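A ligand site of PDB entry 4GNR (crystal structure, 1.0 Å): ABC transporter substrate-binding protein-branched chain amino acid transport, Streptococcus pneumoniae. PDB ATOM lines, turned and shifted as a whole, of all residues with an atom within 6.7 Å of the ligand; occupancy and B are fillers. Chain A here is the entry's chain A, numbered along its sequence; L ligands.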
ATOM      1  N   GLU A  15     -39.446   4.207  27.899  1.00  0.00           N
ATOM      2  CA  GLU A  15     -39.173   4.947  26.658  1.00  0.00           C
ATOM      3  C   GLU A  15     -40.056   4.315  25.556  1.00  0.00           C
ATOM      4  O   GLU A  15     -39.598   3.475  24.773  1.00  0.00           O
ATOM      5  CB  GLU A  15     -37.712   4.832  26.289  1.00  0.00           C
ATOM      6  CG  GLU A  15     -36.676   5.413  27.298  1.00  0.00           C
ATOM      7  CD  GLU A  15     -36.263   4.547  28.495  1.00  0.00           C
ATOM      8  OE1 GLU A  15     -37.049   3.709  28.974  1.00  0.00           O
ATOM      9  OE2 GLU A  15     -35.125   4.770  28.972  1.00  0.00           O
ATOM     10  N   LEU A  20     -35.433   6.356  21.737  1.00  0.00           N
ATOM     11  CA  LEU A  20     -35.074   5.105  22.437  1.00  0.00           C
ATOM     12  C   LEU A  20     -36.270   4.163  22.538  1.00  0.00           C
ATOM     13  O   LEU A  20     -36.242   3.177  23.279  1.00  0.00           O
ATOM     14  CB  LEU A  20     -34.546   5.449  23.842  1.00  0.00           C
ATOM     15  CG  LEU A  20     -33.302   6.356  23.809  1.00  0.00           C
ATOM     16  CD1 LEU A  20     -33.027   6.981  25.171  1.00  0.00           C
ATOM     17  CD2 LEU A  20     -32.055   5.629  23.266  1.00  0.00           C
ATOM     18  N   TYR A  23     -36.322   0.218  22.731  1.00  0.00           N
ATOM     19  CA  TYR A  23     -35.939  -0.393  24.015  1.00  0.00           C
ATOM     20  C   TYR A  23     -37.108  -0.379  25.003  1.00  0.00           C
ATOM     21  O   TYR A  23     -37.444  -1.396  25.600  1.00  0.00           O
ATOM     22  CB  TYR A  23     -34.729   0.323  24.620  1.00  0.00           C
ATOM     23  CG  TYR A  23     -33.523   0.446  23.706  1.00  0.00           C
ATOM     24  CD1 TYR A  23     -33.010  -0.638  22.992  1.00  0.00           C
ATOM     25  CD2 TYR A  23     -32.858   1.656  23.627  1.00  0.00           C
ATOM     26  CE1 TYR A  23     -31.870  -0.517  22.213  1.00  0.00           C
ATOM     27  CE2 TYR A  23     -31.711   1.800  22.840  1.00  0.00           C
ATOM     28  CZ  TYR A  23     -31.216   0.708  22.151  1.00  0.00           C
ATOM     29  OH  TYR A  23     -30.079   0.879  21.371  1.00  0.00           O
ATOM     30  N   GLY A  24     -37.715   0.793  25.193  1.00  0.00           N
ATOM     31  CA  GLY A  24     -38.787   0.910  26.162  1.00  0.00           C
ATOM     32  C   GLY A  24     -40.032   0.154  25.763  1.00  0.00           C
ATOM     33  O   GLY A  24     -40.739  -0.362  26.616  1.00  0.00           O
ATOM     34  N   GLU A  27     -39.557  -3.439  26.604  1.00  0.00           N
ATOM     35  CA  GLU A  27     -39.697  -3.615  28.058  1.00  0.00           C
ATOM     36  C   GLU A  27     -41.151  -3.545  28.485  1.00  0.00           C
ATOM     37  O   GLU A  27     -41.593  -4.322  29.332  1.00  0.00           O
ATOM     38  CB  GLU A  27     -38.783  -2.661  28.810  1.00  0.00           C
ATOM     39  CG  GLU A  27     -37.336  -2.983  28.489  1.00  0.00           C
ATOM     40  CD  GLU A  27     -36.303  -2.350  29.363  1.00  0.00           C
ATOM     41  OE1 GLU A  27     -36.535  -1.755  30.411  1.00  0.00           O
ATOM     42  OE2 GLU A  27     -35.092  -2.519  28.907  1.00  0.00           O
ATOM     43  N   ALA A  83     -35.596   2.152  30.906  1.00  0.00           N
ATOM     44  CA  ALA A  83     -34.718   1.200  30.237  1.00  0.00           C
ATOM     45  C   ALA A  83     -33.265   1.676  30.113  1.00  0.00           C
ATOM     46  O   ALA A  83     -32.327   0.867  30.142  1.00  0.00           O
ATOM     47  CB  ALA A  83     -35.240   0.905  28.813  1.00  0.00           C
ATOM     48  N   THR A  84     -33.088   2.979  29.919  1.00  0.00           N
ATOM     49  CA  THR A  84     -31.781   3.531  29.580  1.00  0.00           C
ATOM     50  C   THR A  84     -31.155   4.279  30.758  1.00  0.00           C
ATOM     51  O   THR A  84     -31.838   4.701  31.707  1.00  0.00           O
ATOM     52  CB  THR A  84     -31.851   4.389  28.295  1.00  0.00           C
ATOM     53  OG1 THR A  84     -32.633   5.562  28.545  1.00  0.00           O
ATOM     54  CG2 THR A  84     -32.384   3.587  27.118  1.00  0.00           C
ATOM     55  N   SER A  85     -29.840   4.465  30.676  1.00  0.00           N
ATOM     56  CA  SER A  85     -29.111   5.012  31.803  1.00  0.00           C
ATOM     57  C   SER A  85     -29.376   6.471  32.128  1.00  0.00           C
ATOM     58  O   SER A  85     -29.527   6.817  33.292  1.00  0.00           O
ATOM     59  CB  SER A  85     -27.606   4.751  31.644  1.00  0.00           C
ATOM     60  OG  SER A  85     -27.293   3.381  31.821  1.00  0.00           O
ATOM     61  N   GLY A  86     -29.410   7.332  31.128  1.00  0.00           N
ATOM     62  CA  GLY A  86     -29.636   8.757  31.405  1.00  0.00           C
ATOM     63  C   GLY A  86     -30.978   8.958  32.099  1.00  0.00           C
ATOM     64  O   GLY A  86     -31.115   9.668  33.093  1.00  0.00           O
ATOM     65  N   SER A 104     -34.486  -0.731  37.166  1.00  0.00           N
ATOM     66  CA  SER A 104     -34.245  -0.643  35.727  1.00  0.00           C
ATOM     67  C   SER A 104     -33.790  -2.013  35.250  1.00  0.00           C
ATOM     68  O   SER A 104     -32.779  -2.535  35.750  1.00  0.00           O
ATOM     69  CB  SER A 104     -33.147   0.343  35.345  1.00  0.00           C
ATOM     70  OG  SER A 104     -32.855   0.193  33.963  1.00  0.00           O
ATOM     71  N   SER A 106     -32.323  -2.728  32.589  1.00  0.00           N
ATOM     72  CA  SER A 106     -31.301  -2.674  31.541  1.00  0.00           C
ATOM     73  C   SER A 106     -30.332  -1.513  31.554  1.00  0.00           C
ATOM     74  O   SER A 106     -29.504  -1.433  30.645  1.00  0.00           O
ATOM     75  CB  SER A 106     -32.068  -2.655  30.189  1.00  0.00           C
ATOM     76  OG  SER A 106     -33.068  -1.640  30.187  1.00  0.00           O
ATOM     77  N   ALA A 107     -30.385  -0.627  32.557  1.00  0.00           N
ATOM     78  CA  ALA A 107     -29.458   0.528  32.594  1.00  0.00           C
ATOM     79  C   ALA A 107     -28.066   0.015  33.034  1.00  0.00           C
ATOM     80  O   ALA A 107     -27.902  -0.412  34.168  1.00  0.00           O
ATOM     81  CB  ALA A 107     -29.966   1.595  33.521  1.00  0.00           C
ATOM     82  N   THR A 108     -27.093   0.115  32.130  1.00  0.00           N
ATOM     83  CA  THR A 108     -25.765  -0.453  32.316  1.00  0.00           C
ATOM     84  C   THR A 108     -24.699   0.509  32.819  1.00  0.00           C
ATOM     85  O   THR A 108     -23.546   0.091  33.044  1.00  0.00           O
ATOM     86  CB  THR A 108     -25.293  -1.079  30.973  1.00  0.00           C
ATOM     87  OG1 THR A 108     -25.368  -0.068  29.954  1.00  0.00           O
ATOM     88  CG2 THR A 108     -26.145  -2.280  30.573  1.00  0.00           C
ATOM     89  N   GLN A 109     -25.021   1.761  33.061  1.00  0.00           N
ATOM     90  CA  GLN A 109     -24.002   2.731  33.508  1.00  0.00           C
ATOM     91  C   GLN A 109     -23.289   2.282  34.764  1.00  0.00           C
ATOM     92  O   GLN A 109     -23.907   1.902  35.750  1.00  0.00           O
ATOM     93  CB  GLN A 109     -24.655   4.100  33.732  1.00  0.00           C
ATOM     94  CG  GLN A 109     -23.764   5.187  34.319  1.00  0.00           C
ATOM     95  CD  GLN A 109     -24.531   6.507  34.487  1.00  0.00           C
ATOM     96  OE1 GLN A 109     -25.182   6.974  33.540  1.00  0.00           O
ATOM     97  NE2 GLN A 109     -24.424   7.136  35.679  1.00  0.00           N
ATOM     98  N   THR A 123     -29.214  -5.822  35.072  1.00  0.00           N
ATOM     99  CA  THR A 123     -28.245  -6.196  34.040  1.00  0.00           C
ATOM    100  C   THR A 123     -26.789  -5.942  34.428  1.00  0.00           C
ATOM    101  O   THR A 123     -26.460  -5.572  35.570  1.00  0.00           O
ATOM    102  CB  THR A 123     -28.641  -5.394  32.740  1.00  0.00           C
ATOM    103  OG1 THR A 123     -27.932  -5.925  31.625  1.00  0.00           O
ATOM    104  CG2 THR A 123     -28.378  -3.913  32.912  1.00  0.00           C
ATOM    105  N   PHE A 124     -25.891  -6.228  33.484  1.00  0.00           N
ATOM    106  CA  PHE A 124     -24.473  -6.011  33.620  1.00  0.00           C
ATOM    107  C   PHE A 124     -24.139  -4.506  33.404  1.00  0.00           C
ATOM    108  O   PHE A 124     -25.020  -3.692  33.158  1.00  0.00           O
ATOM    109  CB  PHE A 124     -23.699  -6.969  32.690  1.00  0.00           C
ATOM    110  CG  PHE A 124     -24.261  -7.054  31.281  1.00  0.00           C
ATOM    111  CD1 PHE A 124     -24.728  -8.262  30.789  1.00  0.00           C
ATOM    112  CD2 PHE A 124     -24.346  -5.927  30.457  1.00  0.00           C
ATOM    113  CE1 PHE A 124     -25.267  -8.360  29.503  1.00  0.00           C
ATOM    114  CE2 PHE A 124     -24.914  -6.023  29.179  1.00  0.00           C
ATOM    115  CZ  PHE A 124     -25.377  -7.228  28.711  1.00  0.00           C
ATOM    116  N   ASP A 126     -21.317  -1.240  31.863  1.00  0.00           N
ATOM    117  CA  ASP A 126     -20.541  -0.825  30.687  1.00  0.00           C
ATOM    118  C   ASP A 126     -19.076  -1.212  30.752  1.00  0.00           C
ATOM    119  O   ASP A 126     -18.499  -1.531  29.707  1.00  0.00           O
ATOM    120  CB  ASP A 126     -20.730   0.657  30.449  1.00  0.00           C
ATOM    121  CG  ASP A 126     -22.162   0.995  30.076  1.00  0.00           C
ATOM    122  OD1 ASP A 126     -22.847   0.120  29.492  1.00  0.00           O
ATOM    123  OD2 ASP A 126     -22.584   2.124  30.368  1.00  0.00           O
ATOM    124  N   GLN A 129     -18.972  -4.640  29.557  1.00  0.00           N
ATOM    125  CA  GLN A 129     -19.165  -4.693  28.116  1.00  0.00           C
ATOM    126  C   GLN A 129     -17.886  -4.342  27.340  1.00  0.00           C
ATOM    127  O   GLN A 129     -17.523  -5.000  26.367  1.00  0.00           O
ATOM    128  CB  GLN A 129     -20.302  -3.794  27.646  1.00  0.00           C
ATOM    129  CG  GLN A 129     -21.660  -4.178  28.206  1.00  0.00           C
ATOM    130  CD  GLN A 129     -22.781  -3.582  27.386  1.00  0.00           C
ATOM    131  OE1 GLN A 129     -23.066  -4.035  26.277  1.00  0.00           O
ATOM    132  NE2 GLN A 129     -23.450  -2.585  27.935  1.00  0.00           N
ATOM    133  N   TYR A 156     -23.320   6.433  28.258  1.00  0.00           N
ATOM    134  CA  TYR A 156     -23.366   4.999  27.982  1.00  0.00           C
ATOM    135  C   TYR A 156     -22.250   4.629  27.010  1.00  0.00           C
ATOM    136  O   TYR A 156     -21.391   3.761  27.278  1.00  0.00           O
ATOM    137  CB  TYR A 156     -24.751   4.655  27.394  1.00  0.00           C
ATOM    138  CG  TYR A 156     -24.801   3.332  26.660  1.00  0.00           C
ATOM    139  CD1 TYR A 156     -24.797   2.136  27.355  1.00  0.00           C
ATOM    140  CD2 TYR A 156     -24.889   3.275  25.271  1.00  0.00           C
ATOM    141  CE1 TYR A 156     -24.840   0.938  26.714  1.00  0.00           C
ATOM    142  CE2 TYR A 156     -24.911   2.072  24.607  1.00  0.00           C
ATOM    143  CZ  TYR A 156     -24.894   0.895  25.331  1.00  0.00           C
ATOM    144  OH  TYR A 156     -24.927  -0.297  24.650  1.00  0.00           O
ATOM    145  N   GLY A 204     -22.980   2.811  21.026  1.00  0.00           N
ATOM    146  CA  GLY A 204     -24.101   3.668  20.708  1.00  0.00           C
ATOM    147  C   GLY A 204     -25.407   2.894  20.656  1.00  0.00           C
ATOM    148  O   GLY A 204     -25.445   1.676  20.852  1.00  0.00           O
ATOM    149  N   TYR A 205     -26.458   3.662  20.416  1.00  0.00           N
ATOM    150  CA  TYR A 205     -27.840   3.182  20.330  1.00  0.00           C
ATOM    151  C   TYR A 205     -28.254   2.855  18.880  1.00  0.00           C
ATOM    152  O   TYR A 205     -27.585   3.255  17.930  1.00  0.00           O
ATOM    153  CB  TYR A 205     -28.799   4.147  20.993  1.00  0.00           C
ATOM    154  CG  TYR A 205     -28.554   4.358  22.482  1.00  0.00           C
ATOM    155  CD1 TYR A 205     -28.505   3.295  23.366  1.00  0.00           C
ATOM    156  CD2 TYR A 205     -28.468   5.620  23.021  1.00  0.00           C
ATOM    157  CE1 TYR A 205     -28.364   3.497  24.726  1.00  0.00           C
ATOM    158  CE2 TYR A 205     -28.348   5.828  24.405  1.00  0.00           C
ATOM    159  CZ  TYR A 205     -28.302   4.767  25.243  1.00  0.00           C
ATOM    160  OH  TYR A 205     -28.191   4.999  26.600  1.00  0.00           O
ATOM    161  N   GLY A 228     -22.175  -2.892  21.635  1.00  0.00           N
ATOM    162  CA  GLY A 228     -22.666  -3.263  22.951  1.00  0.00           C
ATOM    163  C   GLY A 228     -24.159  -3.628  22.855  1.00  0.00           C
ATOM    164  O   GLY A 228     -24.724  -3.843  21.778  1.00  0.00           O
ATOM    165  N   ASP A 229     -24.794  -3.642  24.014  1.00  0.00           N
ATOM    166  CA  ASP A 229     -26.184  -4.073  24.102  1.00  0.00           C
ATOM    167  C   ASP A 229     -27.148  -3.175  23.327  1.00  0.00           C
ATOM    168  O   ASP A 229     -28.274  -3.589  23.032  1.00  0.00           O
ATOM    169  CB  ASP A 229     -26.649  -4.305  25.543  1.00  0.00           C
ATOM    170  CG  ASP A 229     -26.740  -3.034  26.407  1.00  0.00           C
ATOM    171  OD1 ASP A 229     -25.882  -2.123  26.275  1.00  0.00           O
ATOM    172  OD2 ASP A 229     -27.653  -2.995  27.287  1.00  0.00           O
ATOM    173  N   GLY A 230     -26.725  -1.953  22.996  1.00  0.00           N
ATOM    174  CA  GLY A 230     -27.576  -1.078  22.199  1.00  0.00           C
ATOM    175  C   GLY A 230     -27.940  -1.621  20.816  1.00  0.00           C
ATOM    176  O   GLY A 230     -28.889  -1.134  20.190  1.00  0.00           O
ATOM    177  N   PHE A 231     -27.192  -2.600  20.295  1.00  0.00           N
ATOM    178  CA  PHE A 231     -27.506  -3.192  18.982  1.00  0.00           C
ATOM    179  C   PHE A 231     -28.691  -4.159  19.021  1.00  0.00           C
ATOM    180  O   PHE A 231     -29.146  -4.575  17.962  1.00  0.00           O
ATOM    181  CB  PHE A 231     -26.296  -3.963  18.420  1.00  0.00           C
ATOM    182  CG  PHE A 231     -25.218  -3.135  17.760  1.00  0.00           C
ATOM    183  CD1 PHE A 231     -24.860  -1.853  18.177  1.00  0.00           C
ATOM    184  CD2 PHE A 231     -24.435  -3.749  16.780  1.00  0.00           C
ATOM    185  CE1 PHE A 231     -23.783  -1.189  17.549  1.00  0.00           C
ATOM    186  CE2 PHE A 231     -23.389  -3.097  16.171  1.00  0.00           C
ATOM    187  CZ  PHE A 231     -23.064  -1.824  16.560  1.00  0.00           C
ATOM    188  N   PHE A 282     -34.258  -7.049  25.968  1.00  0.00           N
ATOM    189  CA  PHE A 282     -34.861  -6.075  26.871  1.00  0.00           C
ATOM    190  C   PHE A 282     -36.238  -6.515  27.332  1.00  0.00           C
ATOM    191  O   PHE A 282     -36.605  -6.276  28.478  1.00  0.00           O
ATOM    192  CB  PHE A 282     -34.810  -4.689  26.237  1.00  0.00           C
ATOM    193  CG  PHE A 282     -33.397  -4.297  25.905  1.00  0.00           C
ATOM    194  CD1 PHE A 282     -32.423  -4.285  26.902  1.00  0.00           C
ATOM    195  CD2 PHE A 282     -33.001  -3.977  24.631  1.00  0.00           C
ATOM    196  CE1 PHE A 282     -31.088  -4.004  26.620  1.00  0.00           C
ATOM    197  CE2 PHE A 282     -31.670  -3.655  24.336  1.00  0.00           C
ATOM    198  CZ  PHE A 282     -30.714  -3.690  25.325  1.00  0.00           C
HETATM  199  N1  LIG L   1     -27.750  -0.430  28.436  1.00  0.00           N
HETATM  200  C1  LIG L   1     -28.241   0.781  27.727  1.00  0.00           C
HETATM  201  C2  LIG L   1     -28.344   1.938  28.719  1.00  0.00           C
HETATM  202  O1  LIG L   1     -28.713   3.052  28.302  1.00  0.00           O
HETATM  203  C3  LIG L   1     -29.481   0.517  26.820  1.00  0.00           C
HETATM  204  C4  LIG L   1     -30.534  -0.277  27.560  1.00  0.00           C
HETATM  205  C5  LIG L   1     -29.166  -0.251  25.423  1.00  0.00           C
HETATM  206  C6  LIG L   1     -31.790  -0.473  26.735  1.00  0.00           C
HETATM  207  O2  LIG L   1     -28.016   1.712  29.900  1.00  0.00           O
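An oxygen (O1) of the ligand sits at hydrogen-bond distance from the side-chain hydroxyl (OH) of Tyr 205, 2.6 Å away.
The backbone NH (N) of Ser 85 lies within hydrogen-bond range of an oxygen (O1) of the ligand (3.0 Å).
The side-chain hydroxyl (OG) of Ser 85 lies within hydrogen-bond range of an oxygen (O2) of the ligand (2.6 Å).
The side-chain carboxylate (OD2) of Asp 229 is in salt-bridge range of a nitrogen (N1) of the ligand (2.8 Å).
An oxygen (O2) of the ligand is in hydrogen-bond range of the backbone NH (N) of Thr 108 (2.9 Å).
OG1 of Thr 108 lies within hydrogen-bond range of N1 of the ligand (2.8 Å).
The backbone carbonyl oxygen (O) of Ser 106 lies within hydrogen-bond range of a nitrogen (N1) of the ligand.
The side-chain carboxylate (OD1) of Asp 229 sits at hydrogen-bond distance from the side-chain hydroxyl (OH) of Tyr 156 (2.6 Å).
The backbone carbonyl oxygen (O) of Ala 83 lies within hydrogen-bond range of the side-chain hydroxyl (OG) of Ser 106, at 2.6 Å.
The side-chain hydroxyl (OG) of Ser 106 sits at hydrogen-bond distance from the side-chain carboxylate (OE2) of Glu 27 (2.6 Å).
N of Ser 106 sits close to OG of Ser 104, at 3.3 Å.
O of Ala 83 lies within hydrogen-bond range of N of Ala 107 (3.4 Å).
The side-chain carboxylate of Glu 15 lies within hydrogen-bond range of the backbone NH of Ala 83 (2.9 Å).
The backbone NH of Gly 230 is in hydrogen-bond range of the side-chain hydroxyl of Tyr 156, at 3.0 Å.
O of Gly 230 is in hydrogen-bond range of OH of Tyr 23, at 2.6 Å.
Tyr 23 touches the ligand.
Ala 83 touches the ligand (O to C4, 3.3 Å).
CA of Thr 84 touches O1 of the ligand, 3.4 Å away.
Ala 107 touches the ligand.
Tyr 156 touches the ligand (CE1 to C1, 3.6 Å).
Gly 230 touches the ligand.
Phe 282 touches the ligand (CE1 to C6, 3.6 Å).
Hydrophobic or aromatic side chains that line the ligand: Tyr 23, Tyr 156, Tyr 205 and Phe 282.
Within 4 Å of the ligand: Tyr 23, Ala 83, Thr 84, Ser 85, Ser 106, Ala 107, Thr 108, Tyr 156, Tyr 205, Asp 229, Gly 230 and Phe 282.
The nearest printed residue that does not touch the ligand is Gln 109 (4.4 Å).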
